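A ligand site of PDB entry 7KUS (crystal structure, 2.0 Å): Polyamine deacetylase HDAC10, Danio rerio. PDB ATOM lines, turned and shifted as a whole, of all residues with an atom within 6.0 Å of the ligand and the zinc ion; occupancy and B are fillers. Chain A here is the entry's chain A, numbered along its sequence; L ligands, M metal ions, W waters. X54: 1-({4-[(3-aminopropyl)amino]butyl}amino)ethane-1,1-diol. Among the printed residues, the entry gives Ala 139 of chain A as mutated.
The zinc ion is bound by OD2 of Asp 176 (1.9 Å), O04 of the ligand (1.9 Å), OD2 of Asp 269 (2.0 Å) and ND1 of His 178 (2.1 Å). The zinc ion has four donor atoms within binding distance. Slightly farther from the zinc ion lies an oxygen (O03) of the ligand (2.6 Å). Slightly farther from the zinc ion lies OD1 of Asp 176 (2.7 Å).
Water W1 lies within hydrogen-bond range of O of Glu 26 (2.6 Å), N10 of the ligand (2.6 Å) and OE1 of Glu 276 (2.9 Å). Water W2 bridges the side-chain carboxylate (OE2) of Glu 276 (2.5 Å) and a nitrogen (N10) of the ligand (3.5 Å).
Merely in contact with the ligand: Ala 96 (3.7 Å), Pro 136 (3.96 Å), Phe 148 (3.7 Å), Trp 207 (3.7 Å), Glu 276 (3.5 Å) and Gly 307 (3.9 Å). Hydrophobic or aromatic side chains within 4 Å of the ligand: Ala 96, Pro 136, His 138, Phe 148, His 178, Trp 207 and Tyr 309. Of the 25 residues printed, 13 come within 4 Å of the ligand.
The backbone NH (N) of Gly 307 lies within hydrogen-bond range of the side-chain carboxylate (OD1) of Asp 176 (3.0 Å). OE2 of Glu 276 is in hydrogen-bond range of NE2 of His 178 (2.8 Å). The backbone NH (N) of His 138 sits at hydrogen-bond distance from the side-chain sulfur (SG) of Cys 149. The backbone NH of His 138 is in hydrogen-bond range of the side-chain carboxylate of Glu 306, 2.9 Å away. The backbone carbonyl oxygen (O) of Ala 96 lies close to the backbone NH (N) of Gly 147, 3.1 Å away. The backbone carbonyl oxygen (O) of Gly 147 lies within hydrogen-bond range of the side-chain sulfur (SG) of Cys 149. O of Asn 95 lies within hydrogen-bond range of N of Gly 147 (2.9 Å). OD1 of Asn 95 sits at hydrogen-bond distance from NE1 of Trp 207 (3.3 Å).
The nearest printed residue that does not touch the zinc ion is Val 177 (4.1 Å).
OH of Tyr 309 lies close to N05 of the ligand (3.5 Å). A ring nitrogen (NE2) of His 138 lies within hydrogen-bond range of an oxygen (O03) of the ligand (2.7 Å). A nitrogen (N10) of the ligand lies within salt-bridge range of the side-chain carboxylate of Glu 26, at 3.4 Å. O of Gly 147 is in hydrogen-bond range of N05 of the ligand, 3.2 Å away.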
ATOM      1  N   PRO A  25     -38.577 -20.381  21.123  1.00  0.00           N
ATOM      2  CA  PRO A  25     -37.363 -20.614  20.313  1.00  0.00           C
ATOM      3  C   PRO A  25     -36.266 -19.594  20.571  1.00  0.00           C
ATOM      4  O   PRO A  25     -35.080 -19.919  20.448  1.00  0.00           O
ATOM      5  CB  PRO A  25     -37.883 -20.525  18.866  1.00  0.00           C
ATOM      6  CG  PRO A  25     -39.377 -20.634  18.965  1.00  0.00           C
ATOM      7  CD  PRO A  25     -39.759 -20.077  20.306  1.00  0.00           C
ATOM      8  N   GLU A  26     -36.649 -18.380  20.969  1.00  0.00           N
ATOM      9  CA  GLU A  26     -35.657 -17.337  21.224  1.00  0.00           C
ATOM     10  C   GLU A  26     -34.765 -17.692  22.422  1.00  0.00           C
ATOM     11  O   GLU A  26     -33.544 -17.480  22.368  1.00  0.00           O
ATOM     12  CB  GLU A  26     -36.385 -16.012  21.438  1.00  0.00           C
ATOM     13  CG  GLU A  26     -35.468 -14.857  21.749  1.00  0.00           C
ATOM     14  CD  GLU A  26     -36.175 -13.517  21.663  1.00  0.00           C
ATOM     15  OE1 GLU A  26     -37.378 -13.460  21.981  1.00  0.00           O
ATOM     16  OE2 GLU A  26     -35.535 -12.524  21.276  1.00  0.00           O
ATOM     17  N   CYS A  27     -35.349 -18.232  23.489  1.00  0.00           N
ATOM     18  CA  CYS A  27     -34.603 -18.509  24.708  1.00  0.00           C
ATOM     19  C   CYS A  27     -34.142 -19.952  24.860  1.00  0.00           C
ATOM     20  O   CYS A  27     -33.345 -20.235  25.763  1.00  0.00           O
ATOM     21  CB  CYS A  27     -35.435 -18.134  25.949  1.00  0.00           C
ATOM     22  SG  CYS A  27     -35.856 -16.384  26.076  1.00  0.00           S
ATOM     23  N   ILE A  29     -31.986 -21.691  23.590  1.00  0.00           N
ATOM     24  CA  ILE A  29     -30.547 -21.954  23.497  1.00  0.00           C
ATOM     25  C   ILE A  29     -29.830 -21.789  24.833  1.00  0.00           C
ATOM     26  O   ILE A  29     -28.697 -22.264  24.992  1.00  0.00           O
ATOM     27  CB  ILE A  29     -29.879 -21.018  22.480  1.00  0.00           C
ATOM     28  CG1 ILE A  29     -30.164 -19.567  22.860  1.00  0.00           C
ATOM     29  CG2 ILE A  29     -30.370 -21.314  21.065  1.00  0.00           C
ATOM     30  CD1 ILE A  29     -29.323 -18.547  22.079  1.00  0.00           C
ATOM     31  N   ASN A  95     -37.580  -8.367  27.554  1.00  0.00           N
ATOM     32  CA  ASN A  95     -37.083  -8.744  26.231  1.00  0.00           C
ATOM     33  C   ASN A  95     -36.158  -9.949  26.344  1.00  0.00           C
ATOM     34  O   ASN A  95     -35.104  -9.863  26.980  1.00  0.00           O
ATOM     35  CB  ASN A  95     -36.361  -7.534  25.626  1.00  0.00           C
ATOM     36  CG  ASN A  95     -35.899  -7.739  24.204  1.00  0.00           C
ATOM     37  OD1 ASN A  95     -36.013  -8.822  23.627  1.00  0.00           O
ATOM     38  ND2 ASN A  95     -35.363  -6.674  23.613  1.00  0.00           N
ATOM     39  N   ALA A  96     -36.555 -11.078  25.726  1.00  0.00           N
ATOM     40  CA  ALA A  96     -35.685 -12.248  25.566  1.00  0.00           C
ATOM     41  C   ALA A  96     -35.138 -12.767  26.913  1.00  0.00           C
ATOM     42  O   ALA A  96     -33.933 -12.905  27.100  1.00  0.00           O
ATOM     43  CB  ALA A  96     -34.539 -11.937  24.599  1.00  0.00           C
ATOM     44  N   PRO A 136     -26.228 -15.321  32.757  1.00  0.00           N
ATOM     45  CA  PRO A 136     -25.279 -14.282  32.366  1.00  0.00           C
ATOM     46  C   PRO A 136     -25.805 -12.918  32.802  1.00  0.00           C
ATOM     47  O   PRO A 136     -26.919 -12.783  33.315  1.00  0.00           O
ATOM     48  CB  PRO A 136     -25.202 -14.397  30.843  1.00  0.00           C
ATOM     49  CG  PRO A 136     -26.534 -14.963  30.443  1.00  0.00           C
ATOM     50  CD  PRO A 136     -26.971 -15.870  31.601  1.00  0.00           C
ATOM     51  N   GLY A 137     -24.980 -11.894  32.612  1.00  0.00           N
ATOM     52  CA  GLY A 137     -25.336 -10.612  33.173  1.00  0.00           C
ATOM     53  C   GLY A 137     -25.349  -9.384  32.287  1.00  0.00           C
ATOM     54  O   GLY A 137     -26.122  -8.462  32.579  1.00  0.00           O
ATOM     55  N   HIS A 138     -24.569  -9.338  31.195  1.00  0.00           N
ATOM     56  CA  HIS A 138     -24.183  -8.036  30.619  1.00  0.00           C
ATOM     57  C   HIS A 138     -25.328  -7.293  29.934  1.00  0.00           C
ATOM     58  O   HIS A 138     -25.202  -6.085  29.709  1.00  0.00           O
ATOM     59  CB  HIS A 138     -22.976  -8.197  29.663  1.00  0.00           C
ATOM     60  CG  HIS A 138     -23.297  -8.857  28.358  1.00  0.00           C
ATOM     61  ND1 HIS A 138     -22.572  -8.609  27.202  1.00  0.00           N
ATOM     62  CD2 HIS A 138     -24.220  -9.795  28.015  1.00  0.00           C
ATOM     63  CE1 HIS A 138     -23.041  -9.347  26.220  1.00  0.00           C
ATOM     64  NE2 HIS A 138     -24.041 -10.075  26.683  1.00  0.00           N
ATOM     65  N   ALA A 139     -26.432  -7.950  29.620  1.00  0.00           N
ATOM     66  CA  ALA A 139     -27.583  -7.258  29.047  1.00  0.00           C
ATOM     67  C   ALA A 139     -28.559  -6.770  30.109  1.00  0.00           C
ATOM     68  O   ALA A 139     -29.481  -6.027  29.772  1.00  0.00           O
ATOM     69  CB  ALA A 139     -28.328  -8.165  28.067  1.00  0.00           C
ATOM     70  N   GLY A 147     -32.359 -10.307  27.736  1.00  0.00           N
ATOM     71  CA  GLY A 147     -31.404 -11.130  27.013  1.00  0.00           C
ATOM     72  C   GLY A 147     -30.766 -12.220  27.855  1.00  0.00           C
ATOM     73  O   GLY A 147     -29.547 -12.332  27.894  1.00  0.00           O
ATOM     74  N   PHE A 148     -31.590 -13.007  28.544  1.00  0.00           N
ATOM     75  CA  PHE A 148     -31.194 -14.104  29.430  1.00  0.00           C
ATOM     76  C   PHE A 148     -30.547 -13.624  30.716  1.00  0.00           C
ATOM     77  O   PHE A 148     -30.128 -14.466  31.530  1.00  0.00           O
ATOM     78  CB  PHE A 148     -30.217 -15.115  28.777  1.00  0.00           C
ATOM     79  CG  PHE A 148     -30.575 -15.522  27.361  1.00  0.00           C
ATOM     80  CD1 PHE A 148     -31.893 -15.535  26.925  1.00  0.00           C
ATOM     81  CD2 PHE A 148     -29.576 -15.931  26.480  1.00  0.00           C
ATOM     82  CE1 PHE A 148     -32.205 -15.935  25.628  1.00  0.00           C
ATOM     83  CE2 PHE A 148     -29.892 -16.338  25.188  1.00  0.00           C
ATOM     84  CZ  PHE A 148     -31.203 -16.329  24.772  1.00  0.00           C
ATOM     85  N   CYS A 149     -30.416 -12.328  30.932  1.00  0.00           N
ATOM     86  CA  CYS A 149     -29.705 -11.784  32.081  1.00  0.00           C
ATOM     87  C   CYS A 149     -30.674 -11.236  33.125  1.00  0.00           C
ATOM     88  O   CYS A 149     -31.613 -10.496  32.792  1.00  0.00           O
ATOM     89  CB  CYS A 149     -28.730 -10.695  31.649  1.00  0.00           C
ATOM     90  SG  CYS A 149     -27.549 -11.193  30.354  1.00  0.00           S
ATOM     91  N   ASP A 176     -18.161 -11.164  24.283  1.00  0.00           N
ATOM     92  CA  ASP A 176     -19.423 -11.768  23.883  1.00  0.00           C
ATOM     93  C   ASP A 176     -19.835 -11.187  22.535  1.00  0.00           C
ATOM     94  O   ASP A 176     -19.490 -10.046  22.212  1.00  0.00           O
ATOM     95  CB  ASP A 176     -20.474 -11.476  24.962  1.00  0.00           C
ATOM     96  CG  ASP A 176     -21.767 -12.257  24.773  1.00  0.00           C
ATOM     97  OD1 ASP A 176     -21.983 -13.252  25.485  1.00  0.00           O
ATOM     98  OD2 ASP A 176     -22.584 -11.900  23.898  1.00  0.00           O
ATOM     99  N   VAL A 177     -20.569 -11.981  21.744  1.00  0.00           N
ATOM    100  CA  VAL A 177     -20.944 -11.531  20.406  1.00  0.00           C
ATOM    101  C   VAL A 177     -22.121 -10.563  20.419  1.00  0.00           C
ATOM    102  O   VAL A 177     -22.429  -9.960  19.386  1.00  0.00           O
ATOM    103  CB  VAL A 177     -21.260 -12.727  19.492  1.00  0.00           C
ATOM    104  CG1 VAL A 177     -22.731 -13.174  19.654  1.00  0.00           C
ATOM    105  CG2 VAL A 177     -20.931 -12.392  18.026  1.00  0.00           C
ATOM    106  N   HIS A 178     -22.798 -10.397  21.555  1.00  0.00           N
ATOM    107  CA  HIS A 178     -23.854  -9.414  21.721  1.00  0.00           C
ATOM    108  C   HIS A 178     -23.312  -8.206  22.451  1.00  0.00           C
ATOM    109  O   HIS A 178     -22.381  -8.307  23.269  1.00  0.00           O
ATOM    110  CB  HIS A 178     -25.048 -10.005  22.508  1.00  0.00           C
ATOM    111  CG  HIS A 178     -25.664 -11.204  21.868  1.00  0.00           C
ATOM    112  ND1 HIS A 178     -25.266 -12.494  22.149  1.00  0.00           N
ATOM    113  CD2 HIS A 178     -26.659 -11.319  20.943  1.00  0.00           C
ATOM    114  CE1 HIS A 178     -25.991 -13.342  21.453  1.00  0.00           C
ATOM    115  NE2 HIS A 178     -26.842 -12.660  20.704  1.00  0.00           N
ATOM    116  N   HIS A 179     -23.892  -7.053  22.161  1.00  0.00           N
ATOM    117  CA  HIS A 179     -23.568  -5.846  22.920  1.00  0.00           C
ATOM    118  C   HIS A 179     -24.011  -6.014  24.369  1.00  0.00           C
ATOM    119  O   HIS A 179     -25.078  -6.564  24.644  1.00  0.00           O
ATOM    120  CB  HIS A 179     -24.283  -4.634  22.309  1.00  0.00           C
ATOM    121  CG  HIS A 179     -23.830  -3.331  22.862  1.00  0.00           C
ATOM    122  ND1 HIS A 179     -24.681  -2.270  23.096  1.00  0.00           N
ATOM    123  CD2 HIS A 179     -22.606  -2.923  23.263  1.00  0.00           C
ATOM    124  CE1 HIS A 179     -23.985  -1.263  23.594  1.00  0.00           C
ATOM    125  NE2 HIS A 179     -22.731  -1.632  23.697  1.00  0.00           N
ATOM    126  N   TRP A 207     -30.068  -8.302  17.219  1.00  0.00           N
ATOM    127  CA  TRP A 207     -30.401  -8.093  18.625  1.00  0.00           C
ATOM    128  C   TRP A 207     -29.199  -7.546  19.395  1.00  0.00           C
ATOM    129  O   TRP A 207     -28.086  -8.063  19.236  1.00  0.00           O
ATOM    130  CB  TRP A 207     -30.883  -9.429  19.228  1.00  0.00           C
ATOM    131  CG  TRP A 207     -31.519  -9.237  20.547  1.00  0.00           C
ATOM    132  CD1 TRP A 207     -32.849  -9.100  20.800  1.00  0.00           C
ATOM    133  CD2 TRP A 207     -30.849  -9.127  21.808  1.00  0.00           C
ATOM    134  NE1 TRP A 207     -33.058  -8.907  22.154  1.00  0.00           N
ATOM    135  CE2 TRP A 207     -31.844  -8.919  22.785  1.00  0.00           C
ATOM    136  CE3 TRP A 207     -29.508  -9.158  22.207  1.00  0.00           C
ATOM    137  CZ2 TRP A 207     -31.536  -8.763  24.146  1.00  0.00           C
ATOM    138  CZ3 TRP A 207     -29.209  -9.011  23.566  1.00  0.00           C
ATOM    139  CH2 TRP A 207     -30.220  -8.804  24.513  1.00  0.00           C
ATOM    140  N   GLY A 267     -18.203 -13.918  26.667  1.00  0.00           N
ATOM    141  CA  GLY A 267     -19.188 -14.678  25.940  1.00  0.00           C
ATOM    142  C   GLY A 267     -18.490 -15.366  24.792  1.00  0.00           C
ATOM    143  O   GLY A 267     -17.788 -14.726  23.994  1.00  0.00           O
ATOM    144  N   ASP A 269     -20.143 -17.027  22.527  1.00  0.00           N
ATOM    145  CA  ASP A 269     -20.949 -17.030  21.319  1.00  0.00           C
ATOM    146  C   ASP A 269     -20.273 -16.272  20.181  1.00  0.00           C
ATOM    147  O   ASP A 269     -20.846 -16.179  19.085  1.00  0.00           O
ATOM    148  CB  ASP A 269     -22.361 -16.483  21.568  1.00  0.00           C
ATOM    149  CG  ASP A 269     -22.388 -15.203  22.378  1.00  0.00           C
ATOM    150  OD1 ASP A 269     -21.345 -14.540  22.527  1.00  0.00           O
ATOM    151  OD2 ASP A 269     -23.509 -14.858  22.848  1.00  0.00           O
ATOM    152  N   GLU A 276     -26.014 -18.022  17.579  1.00  0.00           N
ATOM    153  CA  GLU A 276     -26.297 -16.589  17.673  1.00  0.00           C
ATOM    154  C   GLU A 276     -25.272 -15.745  16.936  1.00  0.00           C
ATOM    155  O   GLU A 276     -25.634 -14.797  16.225  1.00  0.00           O
ATOM    156  CB  GLU A 276     -26.346 -16.162  19.138  1.00  0.00           C
ATOM    157  CG  GLU A 276     -27.633 -16.492  19.835  1.00  0.00           C
ATOM    158  CD  GLU A 276     -28.778 -15.623  19.351  1.00  0.00           C
ATOM    159  OE1 GLU A 276     -29.771 -16.191  18.869  1.00  0.00           O
ATOM    160  OE2 GLU A 276     -28.683 -14.370  19.458  1.00  0.00           O
ATOM    161  N   GLU A 306     -20.326 -15.164  30.112  1.00  0.00           N
ATOM    162  CA  GLU A 306     -21.609 -14.622  29.678  1.00  0.00           C
ATOM    163  C   GLU A 306     -22.346 -15.628  28.801  1.00  0.00           C
ATOM    164  O   GLU A 306     -22.860 -16.633  29.322  1.00  0.00           O
ATOM    165  CB  GLU A 306     -21.409 -13.288  28.926  1.00  0.00           C
ATOM    166  CG  GLU A 306     -20.691 -12.256  29.775  1.00  0.00           C
ATOM    167  CD  GLU A 306     -21.642 -11.429  30.683  1.00  0.00           C
ATOM    168  OE1 GLU A 306     -22.864 -11.689  30.698  1.00  0.00           O
ATOM    169  OE2 GLU A 306     -21.162 -10.490  31.361  1.00  0.00           O
ATOM    170  N   GLY A 307     -22.394 -15.397  27.482  1.00  0.00           N
ATOM    171  CA  GLY A 307     -23.037 -16.309  26.554  1.00  0.00           C
ATOM    172  C   GLY A 307     -22.092 -17.361  25.994  1.00  0.00           C
ATOM    173  O   GLY A 307     -20.948 -17.503  26.415  1.00  0.00           O
ATOM    174  N   GLY A 308     -22.612 -18.138  25.018  1.00  0.00           N
ATOM    175  CA  GLY A 308     -21.905 -19.253  24.395  1.00  0.00           C
ATOM    176  C   GLY A 308     -22.810 -20.467  24.255  1.00  0.00           C
ATOM    177  O   GLY A 308     -23.131 -21.118  25.257  1.00  0.00           O
ATOM    178  N   TYR A 309     -23.311 -20.757  23.042  1.00  0.00           N
ATOM    179  CA  TYR A 309     -24.465 -21.631  22.924  1.00  0.00           C
ATOM    180  C   TYR A 309     -24.246 -22.895  22.114  1.00  0.00           C
ATOM    181  O   TYR A 309     -25.117 -23.764  22.110  1.00  0.00           O
ATOM    182  CB  TYR A 309     -25.662 -20.853  22.343  1.00  0.00           C
ATOM    183  CG  TYR A 309     -25.898 -19.614  23.162  1.00  0.00           C
ATOM    184  CD1 TYR A 309     -26.493 -19.698  24.400  1.00  0.00           C
ATOM    185  CD2 TYR A 309     -25.450 -18.382  22.730  1.00  0.00           C
ATOM    186  CE1 TYR A 309     -26.682 -18.586  25.183  1.00  0.00           C
ATOM    187  CE2 TYR A 309     -25.630 -17.245  23.498  1.00  0.00           C
ATOM    188  CZ  TYR A 309     -26.241 -17.353  24.727  1.00  0.00           C
ATOM    189  OH  TYR A 309     -26.408 -16.242  25.500  1.00  0.00           O
HETATM  190  C13 X54 L   1     -32.965 -14.754  18.376  1.00  0.00           C
HETATM  191  C01 X54 L   1     -25.696 -13.307  26.943  1.00  0.00           C
HETATM  192  C02 X54 L   1     -26.145 -12.945  25.519  1.00  0.00           C
HETATM  193  C06 X54 L   1     -28.142 -12.985  24.090  1.00  0.00           C
HETATM  194  C07 X54 L   1     -29.678 -12.862  24.041  1.00  0.00           C
HETATM  195  C08 X54 L   1     -30.223 -13.164  22.646  1.00  0.00           C
HETATM  196  C09 X54 L   1     -31.668 -12.707  22.394  1.00  0.00           C
HETATM  197  C11 X54 L   1     -32.726 -12.865  20.217  1.00  0.00           C
HETATM  198  C12 X54 L   1     -33.615 -13.648  19.232  1.00  0.00           C
HETATM  199  N05 X54 L   1     -27.603 -12.964  25.447  1.00  0.00           N
HETATM  200  N10 X54 L   1     -32.325 -13.577  21.427  1.00  0.00           N
HETATM  201  N14 X54 L   1     -33.975 -15.637  17.812  1.00  0.00           N
HETATM  202  O03 X54 L   1     -25.630 -11.680  25.238  1.00  0.00           O
HETATM  203  O04 X54 L   1     -25.543 -13.866  24.673  1.00  0.00           O
HETATM  204 ZN    ZN M   1     -24.010 -13.126  23.729  1.00  0.00          ZN
HETATM  205  O   HOH W   1     -31.954 -16.110  20.847  1.00  0.00           O
HETATM  206  O   HOH W   2     -30.208 -12.447  18.919  1.00  0.00           O
HETATM  207  O   HOH W   3     -30.508 -15.208  16.414  1.00  0.00           O
